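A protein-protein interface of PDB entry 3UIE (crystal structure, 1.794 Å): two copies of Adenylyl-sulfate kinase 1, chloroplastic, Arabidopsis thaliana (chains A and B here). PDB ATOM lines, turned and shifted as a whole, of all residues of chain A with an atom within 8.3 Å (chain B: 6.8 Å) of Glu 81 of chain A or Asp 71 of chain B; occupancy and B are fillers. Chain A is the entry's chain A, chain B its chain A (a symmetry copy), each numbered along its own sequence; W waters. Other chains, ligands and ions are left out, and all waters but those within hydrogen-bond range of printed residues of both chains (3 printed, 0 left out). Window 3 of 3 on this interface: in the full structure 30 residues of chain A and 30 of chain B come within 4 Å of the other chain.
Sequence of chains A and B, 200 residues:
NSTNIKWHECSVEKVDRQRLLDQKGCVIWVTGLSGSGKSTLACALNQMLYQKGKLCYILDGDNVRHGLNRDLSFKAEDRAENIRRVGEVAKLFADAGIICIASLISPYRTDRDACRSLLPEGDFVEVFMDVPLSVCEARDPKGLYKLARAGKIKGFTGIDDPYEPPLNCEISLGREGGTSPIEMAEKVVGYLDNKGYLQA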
ATOM      1  N   ARG A  65      23.908  -3.929  16.704  1.00  0.00           N
ATOM      2  CA  ARG A  65      23.691  -2.498  16.477  1.00  0.00           C
ATOM      3  C   ARG A  65      23.063  -2.214  15.120  1.00  0.00           C
ATOM      4  O   ARG A  65      22.647  -1.088  14.844  1.00  0.00           O
ATOM      5  CB  ARG A  65      24.984  -1.693  16.642  1.00  0.00           C
ATOM      6  CG  ARG A  65      25.299  -1.348  18.095  1.00  0.00           C
ATOM      7  CD  ARG A  65      26.682  -0.692  18.203  1.00  0.00           C
ATOM      8  NE  ARG A  65      26.918  -0.122  19.532  1.00  0.00           N
ATOM      9  CZ  ARG A  65      26.383   1.022  19.945  1.00  0.00           C
ATOM     10  NH1 ARG A  65      25.569   1.705  19.141  1.00  0.00           N
ATOM     11  NH2 ARG A  65      26.639   1.480  21.160  1.00  0.00           N
ATOM     12  N   LEU A  68      18.393  -5.098  16.556  1.00  0.00           N
ATOM     13  CA  LEU A  68      17.748  -4.741  17.817  1.00  0.00           C
ATOM     14  C   LEU A  68      18.161  -3.346  18.277  1.00  0.00           C
ATOM     15  O   LEU A  68      17.331  -2.560  18.727  1.00  0.00           O
ATOM     16  CB  LEU A  68      18.141  -5.744  18.913  1.00  0.00           C
ATOM     17  CG  LEU A  68      17.590  -5.493  20.323  1.00  0.00           C
ATOM     18  CD1 LEU A  68      16.058  -5.500  20.302  1.00  0.00           C
ATOM     19  CD2 LEU A  68      18.116  -6.539  21.311  1.00  0.00           C
ATOM     20  N   ASN A  69      19.454  -3.047  18.176  1.00  0.00           N
ATOM     21  CA  ASN A  69      19.962  -1.787  18.703  1.00  0.00           C
ATOM     22  C   ASN A  69      20.304  -0.762  17.630  1.00  0.00           C
ATOM     23  O   ASN A  69      21.192   0.078  17.809  1.00  0.00           O
ATOM     24  CB  ASN A  69      21.155  -2.036  19.625  1.00  0.00           C
ATOM     25  CG  ASN A  69      20.758  -2.804  20.877  1.00  0.00           C
ATOM     26  OD1 ASN A  69      19.583  -2.879  21.204  1.00  0.00           O
ATOM     27  ND2 ASN A  69      21.739  -3.367  21.583  1.00  0.00           N
ATOM     28  N   ASP A  71      18.755   1.681  16.906  1.00  0.00           N
ATOM     29  CA  ASP A  71      18.353   3.016  17.347  1.00  0.00           C
ATOM     30  C   ASP A  71      19.367   3.679  18.282  1.00  0.00           C
ATOM     31  O   ASP A  71      19.183   4.828  18.686  1.00  0.00           O
ATOM     32  CB  ASP A  71      16.993   2.956  18.036  1.00  0.00           C
ATOM     33  CG  ASP A  71      16.996   2.035  19.233  1.00  0.00           C
ATOM     34  OD1 ASP A  71      17.754   1.045  19.204  1.00  0.00           O
ATOM     35  OD2 ASP A  71      16.262   2.308  20.205  1.00  0.00           O
ATOM     36  N   LEU A  72      20.447   2.973  18.613  1.00  0.00           N
ATOM     37  CA  LEU A  72      21.414   3.486  19.588  1.00  0.00           C
ATOM     38  C   LEU A  72      22.646   4.110  18.953  1.00  0.00           C
ATOM     39  O   LEU A  72      23.163   3.612  17.959  1.00  0.00           O
ATOM     40  CB  LEU A  72      21.856   2.362  20.525  1.00  0.00           C
ATOM     41  CG  LEU A  72      20.694   1.765  21.316  1.00  0.00           C
ATOM     42  CD1 LEU A  72      21.217   0.733  22.299  1.00  0.00           C
ATOM     43  CD2 LEU A  72      19.956   2.872  22.034  1.00  0.00           C
ATOM     44  N   SER A  73      23.119   5.197  19.553  1.00  0.00           N
ATOM     45  CA  SER A  73      24.344   5.854  19.118  1.00  0.00           C
ATOM     46  C   SER A  73      25.514   5.371  19.981  1.00  0.00           C
ATOM     47  O   SER A  73      25.443   4.307  20.602  1.00  0.00           O
ATOM     48  CB  SER A  73      24.203   7.363  19.263  1.00  0.00           C
ATOM     49  OG  SER A  73      24.242   7.744  20.635  1.00  0.00           O
ATOM     50  N   LYS A  75      26.954   7.738  22.180  1.00  0.00           N
ATOM     51  CA  LYS A  75      26.936   8.579  23.370  1.00  0.00           C
ATOM     52  C   LYS A  75      26.932   7.655  24.584  1.00  0.00           C
ATOM     53  O   LYS A  75      26.496   6.511  24.491  1.00  0.00           O
ATOM     54  CB  LYS A  75      25.700   9.473  23.368  1.00  0.00           C
ATOM     55  CG  LYS A  75      25.621  10.387  22.158  1.00  0.00           C
ATOM     56  CD  LYS A  75      24.237  10.987  22.011  1.00  0.00           C
ATOM     57  CE  LYS A  75      24.043  11.591  20.627  1.00  0.00           C
ATOM     58  NZ  LYS A  75      22.640  12.048  20.422  1.00  0.00           N
ATOM     59  N   ALA A  76      27.415   8.140  25.721  1.00  0.00           N
ATOM     60  CA  ALA A  76      27.590   7.275  26.885  1.00  0.00           C
ATOM     61  C   ALA A  76      26.283   6.602  27.292  1.00  0.00           C
ATOM     62  O   ALA A  76      26.260   5.420  27.633  1.00  0.00           O
ATOM     63  CB  ALA A  76      28.175   8.063  28.057  1.00  0.00           C
ATOM     64  N   GLU A  77      25.192   7.352  27.263  1.00  0.00           N
ATOM     65  CA  GLU A  77      23.908   6.800  27.694  1.00  0.00           C
ATOM     66  C   GLU A  77      23.452   5.684  26.756  1.00  0.00           C
ATOM     67  O   GLU A  77      22.761   4.750  27.173  1.00  0.00           O
ATOM     68  CB  GLU A  77      22.837   7.891  27.781  1.00  0.00           C
ATOM     69  CG  GLU A  77      23.324   9.196  28.392  1.00  0.00           C
ATOM     70  CD  GLU A  77      24.187   9.999  27.433  1.00  0.00           C
ATOM     71  OE1 GLU A  77      24.004   9.851  26.206  1.00  0.00           O
ATOM     72  OE2 GLU A  77      25.046  10.775  27.899  1.00  0.00           O
ATOM     73  N   ASP A  78      23.831   5.791  25.487  1.00  0.00           N
ATOM     74  CA  ASP A  78      23.418   4.811  24.493  1.00  0.00           C
ATOM     75  C   ASP A  78      24.296   3.571  24.568  1.00  0.00           C
ATOM     76  O   ASP A  78      23.839   2.474  24.260  1.00  0.00           O
ATOM     77  CB  ASP A  78      23.424   5.414  23.084  1.00  0.00           C
ATOM     78  CG  ASP A  78      22.145   6.197  22.771  1.00  0.00           C
ATOM     79  OD1 ASP A  78      21.374   6.502  23.707  1.00  0.00           O
ATOM     80  OD2 ASP A  78      21.912   6.508  21.584  1.00  0.00           O
ATOM     81  N   ARG A  79      25.554   3.740  24.977  1.00  0.00           N
ATOM     82  CA  ARG A  79      26.409   2.588  25.259  1.00  0.00           C
ATOM     83  C   ARG A  79      25.839   1.784  26.432  1.00  0.00           C
ATOM     84  O   ARG A  79      25.803   0.555  26.396  1.00  0.00           O
ATOM     85  CB  ARG A  79      27.849   3.010  25.574  1.00  0.00           C
ATOM     86  CG  ARG A  79      28.654   3.502  24.374  1.00  0.00           C
ATOM     87  CD  ARG A  79      30.121   3.651  24.755  1.00  0.00           C
ATOM     88  NE  ARG A  79      30.878   4.507  23.847  1.00  0.00           N
ATOM     89  CZ  ARG A  79      31.809   4.073  23.001  1.00  0.00           C
ATOM     90  NH1 ARG A  79      32.098   2.777  22.927  1.00  0.00           N
ATOM     91  NH2 ARG A  79      32.454   4.943  22.227  1.00  0.00           N
ATOM     92  N   ALA A  80      25.394   2.480  27.473  1.00  0.00           N
ATOM     93  CA  ALA A  80      24.786   1.816  28.623  1.00  0.00           C
ATOM     94  C   ALA A  80      23.521   1.035  28.221  1.00  0.00           C
ATOM     95  O   ALA A  80      23.316  -0.107  28.648  1.00  0.00           O
ATOM     96  CB  ALA A  80      24.472   2.829  29.723  1.00  0.00           C
ATOM     97  N   GLU A  81      22.671   1.650  27.400  1.00  0.00           N
ATOM     98  CA  GLU A  81      21.459   0.986  26.925  1.00  0.00           C
ATOM     99  C   GLU A  81      21.798  -0.196  26.014  1.00  0.00           C
ATOM    100  O   GLU A  81      21.169  -1.249  26.089  1.00  0.00           O
ATOM    101  CB  GLU A  81      20.546   1.981  26.193  1.00  0.00           C
ATOM    102  CG  GLU A  81      19.260   1.370  25.659  1.00  0.00           C
ATOM    103  CD  GLU A  81      18.327   0.874  26.750  1.00  0.00           C
ATOM    104  OE1 GLU A  81      18.634   1.020  27.958  1.00  0.00           O
ATOM    105  OE2 GLU A  81      17.267   0.332  26.382  1.00  0.00           O
ATOM    106  N   ASN A  82      22.803  -0.015  25.165  1.00  0.00           N
ATOM    107  CA  ASN A  82      23.287  -1.088  24.304  1.00  0.00           C
ATOM    108  C   ASN A  82      23.675  -2.307  25.147  1.00  0.00           C
ATOM    109  O   ASN A  82      23.252  -3.424  24.879  1.00  0.00           O
ATOM    110  CB  ASN A  82      24.500  -0.593  23.508  1.00  0.00           C
ATOM    111  CG  ASN A  82      25.037  -1.631  22.544  1.00  0.00           C
ATOM    112  OD1 ASN A  82      24.286  -2.234  21.775  1.00  0.00           O
ATOM    113  ND2 ASN A  82      26.343  -1.841  22.575  1.00  0.00           N
ATOM    114  N   ILE A  83      24.492  -2.069  26.170  1.00  0.00           N
ATOM    115  CA  ILE A  83      24.972  -3.125  27.058  1.00  0.00           C
ATOM    116  C   ILE A  83      23.802  -3.732  27.820  1.00  0.00           C
ATOM    117  O   ILE A  83      23.697  -4.954  27.967  1.00  0.00           O
ATOM    118  CB  ILE A  83      26.010  -2.559  28.073  1.00  0.00           C
ATOM    119  CG1 ILE A  83      27.273  -2.090  27.340  1.00  0.00           C
ATOM    120  CG2 ILE A  83      26.322  -3.585  29.166  1.00  0.00           C
ATOM    121  CD1 ILE A  83      28.155  -1.124  28.178  1.00  0.00           C
ATOM    122  N   ARG A  84      22.929  -2.873  28.328  1.00  0.00           N
ATOM    123  CA  ARG A  84      21.786  -3.343  29.091  1.00  0.00           C
ATOM    124  C   ARG A  84      20.936  -4.307  28.266  1.00  0.00           C
ATOM    125  O   ARG A  84      20.588  -5.387  28.736  1.00  0.00           O
ATOM    126  CB  ARG A  84      20.913  -2.175  29.550  1.00  0.00           C
ATOM    127  CG  ARG A  84      19.750  -2.621  30.414  1.00  0.00           C
ATOM    128  CD  ARG A  84      18.715  -1.523  30.611  1.00  0.00           C
ATOM    129  NE  ARG A  84      17.884  -1.291  29.428  1.00  0.00           N
ATOM    130  CZ  ARG A  84      16.796  -1.996  29.115  1.00  0.00           C
ATOM    131  NH1 ARG A  84      16.400  -3.007  29.883  1.00  0.00           N
ATOM    132  NH2 ARG A  84      16.101  -1.693  28.022  1.00  0.00           N
ATOM    133  N   ARG A  85      20.590  -3.912  27.045  1.00  0.00           N
ATOM    134  CA  ARG A  85      19.734  -4.757  26.207  1.00  0.00           C
ATOM    135  C   ARG A  85      20.443  -6.056  25.860  1.00  0.00           C
ATOM    136  O   ARG A  85      19.835  -7.124  25.884  1.00  0.00           O
ATOM    137  CB  ARG A  85      19.321  -4.045  24.918  1.00  0.00           C
ATOM    138  CG  ARG A  85      18.394  -2.859  25.110  1.00  0.00           C
ATOM    139  CD  ARG A  85      18.019  -2.286  23.740  1.00  0.00           C
ATOM    140  NE  ARG A  85      17.391  -0.974  23.827  1.00  0.00           N
ATOM    141  CZ  ARG A  85      17.140  -0.206  22.772  1.00  0.00           C
ATOM    142  NH1 ARG A  85      17.464  -0.624  21.552  1.00  0.00           N
ATOM    143  NH2 ARG A  85      16.574   0.981  22.937  1.00  0.00           N
ATOM    144  N   VAL A  86      21.731  -5.972  25.534  1.00  0.00           N
ATOM    145  CA  VAL A  86      22.474  -7.190  25.225  1.00  0.00           C
ATOM    146  C   VAL A  86      22.515  -8.142  26.423  1.00  0.00           C
ATOM    147  O   VAL A  86      22.358  -9.351  26.254  1.00  0.00           O
ATOM    148  CB  VAL A  86      23.892  -6.910  24.679  1.00  0.00           C
ATOM    149  CG1 VAL A  86      24.685  -8.199  24.587  1.00  0.00           C
ATOM    150  CG2 VAL A  86      23.799  -6.256  23.308  1.00  0.00           C
ATOM    151  N   GLY A  87      22.704  -7.602  27.625  1.00  0.00           N
ATOM    152  CA  GLY A  87      22.652  -8.416  28.840  1.00  0.00           C
ATOM    153  C   GLY A  87      21.314  -9.132  29.005  1.00  0.00           C
ATOM    154  O   GLY A  87      21.255 -10.304  29.381  1.00  0.00           O
ATOM    155  N   GLU A  88      20.224  -8.423  28.740  1.00  0.00           N
ATOM    156  CA  GLU A  88      18.895  -9.022  28.853  1.00  0.00           C
ATOM    157  C   GLU A  88      18.675 -10.110  27.801  1.00  0.00           C
ATOM    158  O   GLU A  88      18.093 -11.159  28.084  1.00  0.00           O
ATOM    159  CB  GLU A  88      17.803  -7.948  28.776  1.00  0.00           C
ATOM    160  CG  GLU A  88      17.764  -7.009  30.017  1.00  0.00           C
ATOM    161  CD  GLU A  88      17.039  -7.602  31.235  1.00  0.00           C
ATOM    162  OE1 GLU A  88      16.765  -8.828  31.293  1.00  0.00           O
ATOM    163  OE2 GLU A  88      16.733  -6.822  32.162  1.00  0.00           O
ATOM    164  N   LEU A 104      31.163  -7.383  22.900  1.00  0.00           N
ATOM    165  CA  LEU A 104      30.882  -5.956  22.804  1.00  0.00           C
ATOM    166  C   LEU A 104      32.006  -5.254  23.533  1.00  0.00           C
ATOM    167  O   LEU A 104      32.515  -5.785  24.521  1.00  0.00           O
ATOM    168  CB  LEU A 104      29.602  -5.635  23.573  1.00  0.00           C
ATOM    169  CG  LEU A 104      28.186  -5.530  23.034  1.00  0.00           C
ATOM    170  CD1 LEU A 104      27.648  -6.884  22.603  1.00  0.00           C
ATOM    171  CD2 LEU A 104      27.320  -4.943  24.139  1.00  0.00           C
ATOM    172  N   TYR A 108      32.013   0.253  30.223  1.00  0.00           N
ATOM    173  CA  TYR A 108      31.682   0.716  31.567  1.00  0.00           C
ATOM    174  C   TYR A 108      31.460  -0.439  32.543  1.00  0.00           C
ATOM    175  O   TYR A 108      30.638  -1.331  32.325  1.00  0.00           O
ATOM    176  CB  TYR A 108      30.453   1.628  31.519  1.00  0.00           C
ATOM    177  CG  TYR A 108      30.549   2.717  30.468  1.00  0.00           C
ATOM    178  CD1 TYR A 108      31.752   3.375  30.216  1.00  0.00           C
ATOM    179  CD2 TYR A 108      29.441   3.075  29.719  1.00  0.00           C
ATOM    180  CE1 TYR A 108      31.831   4.376  29.245  1.00  0.00           C
ATOM    181  CE2 TYR A 108      29.511   4.061  28.751  1.00  0.00           C
ATOM    182  CZ  TYR A 108      30.702   4.707  28.516  1.00  0.00           C
ATOM    183  OH  TYR A 108      30.745   5.687  27.547  1.00  0.00           O
ATOM    184  N   ASP A 111      27.975  -1.017  34.006  1.00  0.00           N
ATOM    185  CA  ASP A 111      27.015  -1.627  33.084  1.00  0.00           C
ATOM    186  C   ASP A 111      27.271  -3.115  32.881  1.00  0.00           C
ATOM    187  O   ASP A 111      26.327  -3.895  32.828  1.00  0.00           O
ATOM    188  CB  ASP A 111      26.978  -0.883  31.754  1.00  0.00           C
ATOM    189  CG  ASP A 111      26.527   0.542  31.912  1.00  0.00           C
ATOM    190  OD1 ASP A 111      25.511   0.764  32.604  1.00  0.00           O
ATOM    191  OD2 ASP A 111      27.193   1.442  31.366  1.00  0.00           O
ATOM    192  N   CYS A 115      24.785  -6.480  34.065  1.00  0.00           N
ATOM    193  CA  CYS A 115      24.470  -7.659  33.264  1.00  0.00           C
ATOM    194  C   CYS A 115      24.737  -8.917  34.074  1.00  0.00           C
ATOM    195  O   CYS A 115      23.974  -9.879  34.019  1.00  0.00           O
ATOM    196  CB  CYS A 115      25.298  -7.695  31.976  1.00  0.00           C
ATOM    197  SG  CYS A 115      24.890  -6.372  30.849  1.00  0.00           S
ATOM    198  N   VAL B  64       8.882 -10.368  28.971  1.00  0.00           N
ATOM    199  CA  VAL B  64       9.871  -9.471  28.380  1.00  0.00           C
ATOM    200  C   VAL B  64       9.705  -8.034  28.869  1.00  0.00           C
ATOM    201  O   VAL B  64      10.667  -7.281  28.931  1.00  0.00           O
ATOM    202  CB  VAL B  64       9.829  -9.511  26.850  1.00  0.00           C
ATOM    203  CG1 VAL B  64      10.949  -8.663  26.262  1.00  0.00           C
ATOM    204  CG2 VAL B  64       9.948 -10.947  26.363  1.00  0.00           C
ATOM    205  N   ARG B  65       8.487  -7.660  29.225  1.00  0.00           N
ATOM    206  CA  ARG B  65       8.248  -6.303  29.722  1.00  0.00           C
ATOM    207  C   ARG B  65       8.796  -6.094  31.126  1.00  0.00           C
ATOM    208  O   ARG B  65       8.844  -4.967  31.620  1.00  0.00           O
ATOM    209  CB  ARG B  65       6.763  -5.931  29.670  1.00  0.00           C
ATOM    210  CG  ARG B  65       6.311  -5.438  28.298  1.00  0.00           C
ATOM    211  CD  ARG B  65       4.789  -5.244  28.273  1.00  0.00           C
ATOM    212  NE  ARG B  65       4.345  -4.540  27.067  1.00  0.00           N
ATOM    213  CZ  ARG B  65       4.479  -3.230  26.891  1.00  0.00           C
ATOM    214  NH1 ARG B  65       5.060  -2.488  27.833  1.00  0.00           N
ATOM    215  NH2 ARG B  65       4.054  -2.658  25.775  1.00  0.00           N
ATOM    216  N   GLY B  67      11.942  -7.333  31.795  1.00  0.00           N
ATOM    217  CA  GLY B  67      13.383  -7.394  31.602  1.00  0.00           C
ATOM    218  C   GLY B  67      13.871  -6.469  30.499  1.00  0.00           C
ATOM    219  O   GLY B  67      14.070  -5.269  30.713  1.00  0.00           O
ATOM    220  N   LEU B  68      14.091  -7.036  29.320  1.00  0.00           N
ATOM    221  CA  LEU B  68      14.552  -6.264  28.168  1.00  0.00           C
ATOM    222  C   LEU B  68      13.706  -5.012  27.965  1.00  0.00           C
ATOM    223  O   LEU B  68      14.231  -3.934  27.694  1.00  0.00           O
ATOM    224  CB  LEU B  68      14.463  -7.117  26.893  1.00  0.00           C
ATOM    225  CG  LEU B  68      14.862  -6.447  25.572  1.00  0.00           C
ATOM    226  CD1 LEU B  68      16.319  -5.974  25.638  1.00  0.00           C
ATOM    227  CD2 LEU B  68      14.663  -7.401  24.390  1.00  0.00           C
ATOM    228  N   ASN B  69      12.388  -5.160  28.080  1.00  0.00           N
ATOM    229  CA  ASN B  69      11.493  -4.050  27.782  1.00  0.00           C
ATOM    230  C   ASN B  69      10.878  -3.403  29.017  1.00  0.00           C
ATOM    231  O   ASN B  69       9.766  -2.869  28.971  1.00  0.00           O
ATOM    232  CB  ASN B  69      10.412  -4.485  26.794  1.00  0.00           C
ATOM    233  CG  ASN B  69      10.993  -4.841  25.434  1.00  0.00           C
ATOM    234  OD1 ASN B  69      12.121  -4.479  25.134  1.00  0.00           O
ATOM    235  ND2 ASN B  69      10.218  -5.542  24.605  1.00  0.00           N
ATOM    236  N   ARG B  70      11.621  -3.447  30.112  1.00  0.00           N
ATOM    237  CA  ARG B  70      11.147  -2.881  31.366  1.00  0.00           C
ATOM    238  C   ARG B  70      11.003  -1.367  31.262  1.00  0.00           C
ATOM    239  O   ARG B  70      10.362  -0.737  32.111  1.00  0.00           O
ATOM    240  CB  ARG B  70      12.084  -3.267  32.523  1.00  0.00           C
ATOM    241  CG  ARG B  70      13.473  -2.636  32.465  1.00  0.00           C
ATOM    242  CD  ARG B  70      14.336  -3.074  33.660  1.00  0.00           C
ATOM    243  NE  ARG B  70      14.448  -4.530  33.750  1.00  0.00           N
ATOM    244  CZ  ARG B  70      14.980  -5.185  34.781  1.00  0.00           C
ATOM    245  NH1 ARG B  70      15.448  -4.521  35.827  1.00  0.00           N
ATOM    246  NH2 ARG B  70      15.041  -6.509  34.772  1.00  0.00           N
ATOM    247  N   ASP B  71      11.599  -0.777  30.231  1.00  0.00           N
ATOM    248  CA  ASP B  71      11.546   0.674  30.060  1.00  0.00           C
ATOM    249  C   ASP B  71      10.346   1.145  29.235  1.00  0.00           C
ATOM    250  O   ASP B  71      10.145   2.348  29.058  1.00  0.00           O
ATOM    251  CB  ASP B  71      12.833   1.176  29.413  1.00  0.00           C
ATOM    252  CG  ASP B  71      13.084   0.541  28.066  1.00  0.00           C
ATOM    253  OD1 ASP B  71      12.679  -0.624  27.886  1.00  0.00           O
ATOM    254  OD2 ASP B  71      13.665   1.208  27.185  1.00  0.00           O
ATOM    255  N   LEU B  72       9.534   0.209  28.745  1.00  0.00           N
ATOM    256  CA  LEU B  72       8.425   0.564  27.854  1.00  0.00           C
ATOM    257  C   LEU B  72       7.079   0.637  28.555  1.00  0.00           C
ATOM    258  O   LEU B  72       6.776  -0.175  29.423  1.00  0.00           O
ATOM    259  CB  LEU B  72       8.332  -0.446  26.710  1.00  0.00           C
ATOM    260  CG  LEU B  72       9.599  -0.487  25.857  1.00  0.00           C
ATOM    261  CD1 LEU B  72       9.398  -1.429  24.683  1.00  0.00           C
ATOM    262  CD2 LEU B  72       9.927   0.909  25.381  1.00  0.00           C
ATOM    263  N   SER B  73       6.270   1.612  28.155  1.00  0.00           N
ATOM    264  CA  SER B  73       4.914   1.755  28.667  1.00  0.00           C
ATOM    265  C   SER B  73       3.930   1.098  27.694  1.00  0.00           C
ATOM    266  O   SER B  73       4.314   0.246  26.888  1.00  0.00           O
ATOM    267  CB  SER B  73       4.567   3.230  28.811  1.00  0.00           C
ATOM    268  OG  SER B  73       4.368   3.828  27.534  1.00  0.00           O
ATOM    269  N   ASP B  78       5.225   3.047  22.417  1.00  0.00           N
ATOM    270  CA  ASP B  78       5.957   2.080  23.223  1.00  0.00           C
ATOM    271  C   ASP B  78       5.513   0.664  22.891  1.00  0.00           C
ATOM    272  O   ASP B  78       6.302  -0.271  23.003  1.00  0.00           O
ATOM    273  CB  ASP B  78       5.804   2.376  24.720  1.00  0.00           C
ATOM    274  CG  ASP B  78       6.779   3.449  25.211  1.00  0.00           C
ATOM    275  OD1 ASP B  78       7.386   4.152  24.373  1.00  0.00           O
ATOM    276  OD2 ASP B  78       6.939   3.591  26.443  1.00  0.00           O
ATOM    277  N   GLU B  81       7.574  -0.083  19.801  1.00  0.00           N
ATOM    278  CA  GLU B  81       8.948  -0.406  20.180  1.00  0.00           C
ATOM    279  C   GLU B  81       9.027  -1.784  20.844  1.00  0.00           C
ATOM    280  O   GLU B  81       9.953  -2.551  20.593  1.00  0.00           O
ATOM    281  CB  GLU B  81       9.522   0.670  21.113  1.00  0.00           C
ATOM    282  CG  GLU B  81      10.951   0.408  21.563  1.00  0.00           C
ATOM    283  CD  GLU B  81      11.959   0.445  20.427  1.00  0.00           C
ATOM    284  OE1 GLU B  81      11.584   0.709  19.259  1.00  0.00           O
ATOM    285  OE2 GLU B  81      13.146   0.207  20.720  1.00  0.00           O
ATOM    286  N   ARG B  85      11.314  -4.666  19.176  1.00  0.00           N
ATOM    287  CA  ARG B  85      12.417  -5.340  19.866  1.00  0.00           C
ATOM    288  C   ARG B  85      12.165  -6.837  19.943  1.00  0.00           C
ATOM    289  O   ARG B  85      13.078  -7.634  19.739  1.00  0.00           O
ATOM    290  CB  ARG B  85      12.624  -4.788  21.278  1.00  0.00           C
ATOM    291  CG  ARG B  85      13.122  -3.356  21.339  1.00  0.00           C
ATOM    292  CD  ARG B  85      13.340  -2.960  22.802  1.00  0.00           C
ATOM    293  NE  ARG B  85      13.519  -1.525  22.981  1.00  0.00           N
ATOM    294  CZ  ARG B  85      13.546  -0.929  24.168  1.00  0.00           C
ATOM    295  NH1 ARG B  85      13.408  -1.647  25.278  1.00  0.00           N
ATOM    296  NH2 ARG B  85      13.704   0.385  24.245  1.00  0.00           N
HETATM  297  O   HOH W   1      13.798   2.518  22.245  1.00  0.00           O
HETATM  298  O   HOH W   2      17.596  -4.244  32.307  1.00  0.00           O
HETATM  299  O   HOH W   3      15.873   2.562  25.296  1.00  0.00           O
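The guanidinium group (NH1) of Arg 84 of chain A sits at hydrogen-bond distance from the backbone carbonyl oxygen (O) of Gly 67 of chain B, 3.4 Å away.
NH2 of Arg 84 of chain A sits at hydrogen-bond distance from O of Leu 68 of chain B (2.9 Å).
OD1 of Asp 71 of chain B is in salt-bridge range of NH2 of Arg 84 of chain A (3.6 Å).
NH2 of Arg 70 of chain B is in salt-bridge range of OE2 of Glu 88 of chain A.
NH2 of Arg 85 of chain A lies close to NH2 of Arg 85 of chain B.
O of Gly 67 of chain B sits close to OE2 of Glu 88 of chain A (3.4 Å).
Water W3 lies within hydrogen-bond range of the side-chain carboxylate of Glu 81 of chain A, the guanidinium group of Arg 85 of chain A, the side-chain carboxylate of Asp 71 of chain B and the guanidinium group of Arg 85 of chain B.
Water W1 lies within hydrogen-bond range of OE2 of Glu 81 of chain B (2.8 Å), NH2 of Arg 85 of chain B (2.9 Å), OD2 of Asp 71 of chain A (3.2 Å) and NH2 of Arg 85 of chain A (3.2 Å).
Of the 12 printed residues of chain B, 6 touch a printed residue of chain A.
Hydrophobic or aromatic side chains of chain B that line the printed part of chain A: Leu 68.
Along chain B the printed residues that touch a printed residue of chain A span positions 67 to 85.
Hydrophobic or aromatic side chains of chain A that line the printed part of chain B: Leu 68.
Among the printed residues, 13 pairs touch across the chains.
Among the printed residues, Asp or Glu carboxylates within 4 Å of a Lys or Arg side-chain nitrogen of the other chain: Arg 84 of chain A with Asp 71 of chain B (3.6 Å) and Glu 88 of chain A with Arg 70 of chain B (3.1 Å).
Asp 71 of chain A touches Glu 81 of chain B, and with the chains exchanged Glu 81 of chain A touches Asp 71 of chain B.
Arg 85 of chain B touches its own counterpart, Arg 85 of chain A.
Of the 13 pairs that touch across the chains among the printed residues, 5 have their exchanged pair printed and touching as well.
Of chain B, only Asp 71 (3.8 Å) comes within 4 Å of Glu 81 of chain A.
Printed residues of chain A within 4 Å of Asp 71 of chain B: Glu 81 and Arg 84.
Printed residues of chain A within 4 Å of Arg 70 of chain B: Arg 84 and Glu 88.
Printed residues of chain A within 4 Å of Leu 68 of chain B: Arg 84 (2.9 Å), Arg 85 (3.6 Å) and Glu 88 (3.6 Å).
Leu 72 of chain A touches none of the printed residues of chain B.
The nearest residue of chain B that does not touch Glu 81 of chain A is Arg 85 of chain B (4.2 Å).
The nearest printed residue of chain A that does not touch Gly 67 of chain B is Arg 85 of chain A (7.3 Å).
Leu 68 of chain A touches Arg 85 of chain B (CD1 to CB, 3.6 Å).
Asp 71 of chain A touches Glu 81 of chain B.
Asp 71 of chain B touches Glu 81 of chain A (OD2 to OE2, 3.8 Å).
NH2 of Arg 84 of chain A touches NH1 of Arg 85 of chain B, 3.8 Å away.
Leu 68 of chain B touches Arg 85 of chain A.
N of Leu 68 of chain B touches CD of Glu 88 of chain A, 3.6 Å away.
OD1 of Asn 69 of chain A sits close to NH1 of Arg 85 of chain A (3.1 Å).
The side-chain carboxylate (OE1) of Glu 81 of chain A is in salt-bridge range of the guanidinium group (NE) of Arg 84 of chain A.
The side-chain amide oxygen (OD1) of Asn 69 of chain B lies close to the guanidinium group (NH1) of Arg 85 of chain B.
OD1 of Asp 71 of chain B lies within salt-bridge range of NH1 of Arg 85 of chain B (2.9 Å).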
